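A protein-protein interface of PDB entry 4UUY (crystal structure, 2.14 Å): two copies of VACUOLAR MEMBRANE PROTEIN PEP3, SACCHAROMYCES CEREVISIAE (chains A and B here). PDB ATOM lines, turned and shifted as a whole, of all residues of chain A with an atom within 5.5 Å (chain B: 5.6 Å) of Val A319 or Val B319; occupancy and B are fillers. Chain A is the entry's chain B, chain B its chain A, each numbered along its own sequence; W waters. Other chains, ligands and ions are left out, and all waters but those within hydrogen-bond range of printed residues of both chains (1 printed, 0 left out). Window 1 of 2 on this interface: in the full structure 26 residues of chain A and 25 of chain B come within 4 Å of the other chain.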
ATOM      1  N   SER A  27      -2.535   4.820 -23.367  1.00  0.00           N
ATOM      2  CA  SER A  27      -2.154   6.148 -22.881  1.00  0.00           C
ATOM      3  C   SER A  27      -3.296   7.094 -23.009  1.00  0.00           C
ATOM      4  O   SER A  27      -3.879   7.169 -24.065  1.00  0.00           O
ATOM      5  CB  SER A  27      -0.950   6.684 -23.647  1.00  0.00           C
ATOM      6  OG  SER A  27      -0.432   7.806 -22.948  1.00  0.00           O
ATOM      7  N   ASN A  28      -3.654   7.772 -21.913  1.00  0.00           N
ATOM      8  CA  ASN A  28      -4.724   8.767 -21.919  1.00  0.00           C
ATOM      9  C   ASN A  28      -6.026   8.224 -22.510  1.00  0.00           C
ATOM     10  O   ASN A  28      -6.702   8.885 -23.308  1.00  0.00           O
ATOM     11  CB  ASN A  28      -4.281  10.024 -22.674  1.00  0.00           C
ATOM     12  CG  ASN A  28      -5.187  11.218 -22.397  1.00  0.00           C
ATOM     13  OD1 ASN A  28      -5.667  11.390 -21.271  1.00  0.00           O
ATOM     14  ND2 ASN A  28      -5.435  12.035 -23.415  1.00  0.00           N
ATOM     15  N   PRO A  71       4.338   9.402 -22.329  1.00  0.00           N
ATOM     16  CA  PRO A  71       3.495   9.112 -21.163  1.00  0.00           C
ATOM     17  C   PRO A  71       2.016   9.461 -21.409  1.00  0.00           C
ATOM     18  O   PRO A  71       1.142   8.644 -21.117  1.00  0.00           O
ATOM     19  CB  PRO A  71       4.132   9.959 -20.075  1.00  0.00           C
ATOM     20  CG  PRO A  71       5.595   9.956 -20.439  1.00  0.00           C
ATOM     21  CD  PRO A  71       5.586  10.085 -21.943  1.00  0.00           C
ATOM     22  N   MET A  72       1.763  10.592 -22.077  1.00  0.00           N
ATOM     23  CA  MET A  72       0.398  11.052 -22.344  1.00  0.00           C
ATOM     24  C   MET A  72      -0.163  10.774 -23.735  1.00  0.00           C
ATOM     25  O   MET A  72      -1.245  11.248 -24.070  1.00  0.00           O
ATOM     26  CB  MET A  72       0.347  12.513 -22.102  1.00  0.00           C
ATOM     27  CG  MET A  72       0.965  12.867 -20.769  1.00  0.00           C
ATOM     28  SD  MET A  72       0.458  14.517 -20.379  1.00  0.00           S
ATOM     29  CE  MET A  72      -1.291  14.234 -20.030  1.00  0.00           C
ATOM     30  N   ASP A 317      -1.738   2.385 -18.223  1.00  0.00           N
ATOM     31  CA  ASP A 317      -2.033   3.744 -18.732  1.00  0.00           C
ATOM     32  C   ASP A 317      -1.678   4.703 -17.615  1.00  0.00           C
ATOM     33  O   ASP A 317      -2.415   4.786 -16.607  1.00  0.00           O
ATOM     34  CB  ASP A 317      -3.513   3.872 -19.105  1.00  0.00           C
ATOM     35  CG  ASP A 317      -3.877   5.246 -19.633  1.00  0.00           C
ATOM     36  OD1 ASP A 317      -3.137   6.229 -19.462  1.00  0.00           O
ATOM     37  OD2 ASP A 317      -4.962   5.342 -20.216  1.00  0.00           O
ATOM     38  N   SER A 318      -0.511   5.345 -17.727  1.00  0.00           N
ATOM     39  CA  SER A 318      -0.027   6.217 -16.639  1.00  0.00           C
ATOM     40  C   SER A 318      -0.844   7.495 -16.450  1.00  0.00           C
ATOM     41  O   SER A 318      -0.744   8.154 -15.427  1.00  0.00           O
ATOM     42  CB  SER A 318       1.449   6.552 -16.823  1.00  0.00           C
ATOM     43  OG  SER A 318       2.214   5.378 -16.750  1.00  0.00           O
ATOM     44  N   VAL A 319      -1.665   7.865 -17.414  1.00  0.00           N
ATOM     45  CA  VAL A 319      -2.546   9.015 -17.216  1.00  0.00           C
ATOM     46  C   VAL A 319      -3.813   8.627 -16.464  1.00  0.00           C
ATOM     47  O   VAL A 319      -4.273   9.364 -15.567  1.00  0.00           O
ATOM     48  CB  VAL A 319      -2.954   9.674 -18.555  1.00  0.00           C
ATOM     49  CG1 VAL A 319      -3.814  10.899 -18.294  1.00  0.00           C
ATOM     50  CG2 VAL A 319      -1.724  10.057 -19.362  1.00  0.00           C
ATOM     51  N   LYS A 320      -4.387   7.487 -16.827  1.00  0.00           N
ATOM     52  CA  LYS A 320      -5.676   7.066 -16.305  1.00  0.00           C
ATOM     53  C   LYS A 320      -5.565   6.059 -15.168  1.00  0.00           C
ATOM     54  O   LYS A 320      -6.563   5.695 -14.548  1.00  0.00           O
ATOM     55  CB  LYS A 320      -6.524   6.463 -17.432  1.00  0.00           C
ATOM     56  CG  LYS A 320      -6.763   7.433 -18.570  1.00  0.00           C
ATOM     57  CD  LYS A 320      -7.792   8.464 -18.157  1.00  0.00           C
ATOM     58  CE  LYS A 320      -7.817   9.638 -19.094  1.00  0.00           C
ATOM     59  NZ  LYS A 320      -8.686  10.733 -18.572  1.00  0.00           N
ATOM     60  N   GLU A 321      -4.350   5.608 -14.902  1.00  0.00           N
ATOM     61  CA  GLU A 321      -4.117   4.595 -13.900  1.00  0.00           C
ATOM     62  C   GLU A 321      -5.055   3.384 -14.076  1.00  0.00           C
ATOM     63  O   GLU A 321      -5.819   2.984 -13.162  1.00  0.00           O
ATOM     64  CB  GLU A 321      -4.245   5.216 -12.525  1.00  0.00           C
ATOM     65  CG  GLU A 321      -3.204   4.657 -11.606  1.00  0.00           C
ATOM     66  CD  GLU A 321      -3.231   5.277 -10.247  1.00  0.00           C
ATOM     67  OE1 GLU A 321      -4.013   4.817  -9.391  1.00  0.00           O
ATOM     68  OE2 GLU A 321      -2.405   6.175 -10.049  1.00  0.00           O
ATOM     69  N   SER B  27     -12.858  11.488  -7.358  1.00  0.00           N
ATOM     70  CA  SER B  27     -11.543  10.973  -7.041  1.00  0.00           C
ATOM     71  C   SER B  27     -11.473   9.517  -7.376  1.00  0.00           C
ATOM     72  O   SER B  27     -12.334   8.764  -6.962  1.00  0.00           O
ATOM     73  CB  SER B  27     -11.235  11.217  -5.565  1.00  0.00           C
ATOM     74  OG  SER B  27      -9.856  11.016  -5.398  1.00  0.00           O
ATOM     75  N   ASN B  28     -10.489   9.135  -8.199  1.00  0.00           N
ATOM     76  CA  ASN B  28     -10.307   7.755  -8.589  1.00  0.00           C
ATOM     77  C   ASN B  28     -11.576   7.110  -9.164  1.00  0.00           C
ATOM     78  O   ASN B  28     -11.930   5.960  -8.823  1.00  0.00           O
ATOM     79  CB  ASN B  28      -9.781   6.942  -7.382  1.00  0.00           C
ATOM     80  CG  ASN B  28      -9.182   5.603  -7.792  1.00  0.00           C
ATOM     81  OD1 ASN B  28      -8.562   5.487  -8.839  1.00  0.00           O
ATOM     82  ND2 ASN B  28      -9.410   4.571  -6.974  1.00  0.00           N
ATOM     83  N   PRO B  71      -6.513  13.251  -2.350  1.00  0.00           N
ATOM     84  CA  PRO B  71      -6.295  13.196  -3.806  1.00  0.00           C
ATOM     85  C   PRO B  71      -6.829  11.908  -4.452  1.00  0.00           C
ATOM     86  O   PRO B  71      -7.497  11.975  -5.467  1.00  0.00           O
ATOM     87  CB  PRO B  71      -4.779  13.315  -3.922  1.00  0.00           C
ATOM     88  CG  PRO B  71      -4.404  14.171  -2.746  1.00  0.00           C
ATOM     89  CD  PRO B  71      -5.288  13.663  -1.638  1.00  0.00           C
ATOM     90  N   MET B  72      -6.626  10.763  -3.803  1.00  0.00           N
ATOM     91  CA  MET B  72      -7.040   9.476  -4.358  1.00  0.00           C
ATOM     92  C   MET B  72      -8.353   8.906  -3.824  1.00  0.00           C
ATOM     93  O   MET B  72      -8.677   7.749  -4.101  1.00  0.00           O
ATOM     94  CB  MET B  72      -5.946   8.481  -4.106  1.00  0.00           C
ATOM     95  CG  MET B  72      -4.600   9.011  -4.548  1.00  0.00           C
ATOM     96  SD  MET B  72      -3.448   7.655  -4.632  1.00  0.00           S
ATOM     97  CE  MET B  72      -4.127   6.775  -6.067  1.00  0.00           C
ATOM     98  N   ASP B 317     -10.826  15.229 -11.180  1.00  0.00           N
ATOM     99  CA  ASP B 317     -10.399  13.946 -10.627  1.00  0.00           C
ATOM    100  C   ASP B 317      -8.910  13.849 -10.924  1.00  0.00           C
ATOM    101  O   ASP B 317      -8.528  13.594 -12.072  1.00  0.00           O
ATOM    102  CB  ASP B 317     -11.175  12.799 -11.261  1.00  0.00           C
ATOM    103  CG  ASP B 317     -10.776  11.415 -10.715  1.00  0.00           C
ATOM    104  OD1 ASP B 317      -9.712  11.255 -10.085  1.00  0.00           O
ATOM    105  OD2 ASP B 317     -11.530  10.490 -10.978  1.00  0.00           O
ATOM    106  N   SER B 318      -8.070  14.129  -9.918  1.00  0.00           N
ATOM    107  CA  SER B 318      -6.622  14.151 -10.137  1.00  0.00           C
ATOM    108  C   SER B 318      -6.009  12.761 -10.395  1.00  0.00           C
ATOM    109  O   SER B 318      -4.898  12.672 -10.863  1.00  0.00           O
ATOM    110  CB  SER B 318      -5.911  14.835  -8.965  1.00  0.00           C
ATOM    111  OG  SER B 318      -6.317  16.176  -8.869  1.00  0.00           O
ATOM    112  N   VAL B 319      -6.725  11.683 -10.111  1.00  0.00           N
ATOM    113  CA  VAL B 319      -6.224  10.360 -10.475  1.00  0.00           C
ATOM    114  C   VAL B 319      -6.511  10.026 -11.942  1.00  0.00           C
ATOM    115  O   VAL B 319      -5.665   9.478 -12.641  1.00  0.00           O
ATOM    116  CB  VAL B 319      -6.814   9.249  -9.577  1.00  0.00           C
ATOM    117  CG1 VAL B 319      -6.209   7.894  -9.936  1.00  0.00           C
ATOM    118  CG2 VAL B 319      -6.579   9.560  -8.107  1.00  0.00           C
ATOM    119  N   LYS B 320      -7.712  10.335 -12.390  1.00  0.00           N
ATOM    120  CA  LYS B 320      -8.176   9.939 -13.707  1.00  0.00           C
ATOM    121  C   LYS B 320      -8.031  11.064 -14.732  1.00  0.00           C
ATOM    122  O   LYS B 320      -8.284  10.870 -15.897  1.00  0.00           O
ATOM    123  CB  LYS B 320      -9.638   9.488 -13.619  1.00  0.00           C
ATOM    124  CG  LYS B 320      -9.856   8.326 -12.653  1.00  0.00           C
ATOM    125  CD  LYS B 320      -9.360   7.038 -13.286  1.00  0.00           C
ATOM    126  CE  LYS B 320      -9.233   5.928 -12.280  1.00  0.00           C
ATOM    127  NZ  LYS B 320      -8.572   4.730 -12.892  1.00  0.00           N
ATOM    128  N   GLU B 321      -7.677  12.254 -14.285  1.00  0.00           N
ATOM    129  CA  GLU B 321      -7.606  13.417 -15.155  1.00  0.00           C
ATOM    130  C   GLU B 321      -8.885  13.585 -15.974  1.00  0.00           C
ATOM    131  O   GLU B 321      -8.874  13.660 -17.226  1.00  0.00           O
ATOM    132  CB  GLU B 321      -6.368  13.314 -16.044  1.00  0.00           C
ATOM    133  CG  GLU B 321      -5.722  14.646 -16.194  1.00  0.00           C
ATOM    134  CD  GLU B 321      -4.449  14.611 -16.979  1.00  0.00           C
ATOM    135  OE1 GLU B 321      -4.498  14.666 -18.211  1.00  0.00           O
ATOM    136  OE2 GLU B 321      -3.404  14.576 -16.343  1.00  0.00           O
HETATM  137  O   HOH W   1      -6.346  13.451 -19.608  1.00  0.00           O
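The backbone carbonyl oxygen (O) of Val B319 sits close to the backbone carbonyl oxygen (O) of Val A319 (3.2 Å). NZ of Lys A320 sits at hydrogen-bond distance from O of Glu B321 (3.2 Å). The side-chain amino group (NZ) of Lys A320 is in hydrogen-bond range of the backbone carbonyl oxygen (O) of Lys B320. The side-chain amino group (NZ) of Lys B320 is in hydrogen-bond range of the backbone carbonyl oxygen (O) of Glu A321.
N of Val B319 sits at hydrogen-bond distance from OD1 of Asp B317, at 3.0 Å. The backbone NH (N) of Val A319 lies within hydrogen-bond range of the side-chain carboxylate (OD1) of Asp A317 (3.0 Å). N of Lys A320 lies within hydrogen-bond range of OD1 of Asp A317 (3.2 Å). OD1 of Asp B317 is in hydrogen-bond range of N of Lys B320, 3.2 Å away.
Among the printed residues, merely in contact across the chains: Met A72 with Glu B321 (3.7 Å), Glu A321 with Val B319 (3.8 Å), Val A319 with Glu B321 (3.8 Å) and Glu A321 with Met B72 (3.9 Å).
Val A319 touches just these residues of chain B: Val B319 and Glu B321. Val B319 touches just these residues of chain A: Val A319 and Glu A321. Of the printed residues of chain A, Met B72 touches Glu A321. Printed residues of chain B within 4 Å of Glu A321: Met B72, Val B319 and Lys B320. Asp A317 touches none of the printed residues of chain B. The nearest residue of chain A that does not touch Val B319 is Lys A320 (4.3 Å). The nearest printed residue of chain B that does not touch Glu A321 is Asn B28 (4.6 Å).
Hydrophobic or aromatic side chains of chain B within 4 Å of the printed part of chain A: Met B72 and Val B319. Hydrophobic or aromatic side chains of chain A within 4 Å of the printed part of chain B: Met A72 and Val A319.
Met A72 touches Glu B321, and with the chains exchanged Glu A321 touches Met B72. Val B319 touches its own counterpart, Val A319. Val A319 touches Glu B321, and with the chains exchanged Glu A321 touches Val B319. Lys A320 touches Glu B321, and with the chains exchanged Glu A321 touches Lys B320. 9 positions are printed for both chains. Of the 8 pairs that touch across the chains among the printed residues, 8 have their exchanged pair printed and touching as well.
Water W1 bridges the side-chain carboxylate of Glu B321 (2.6 Å) and the side-chain amide oxygen of Asn A28 (2.7 Å).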
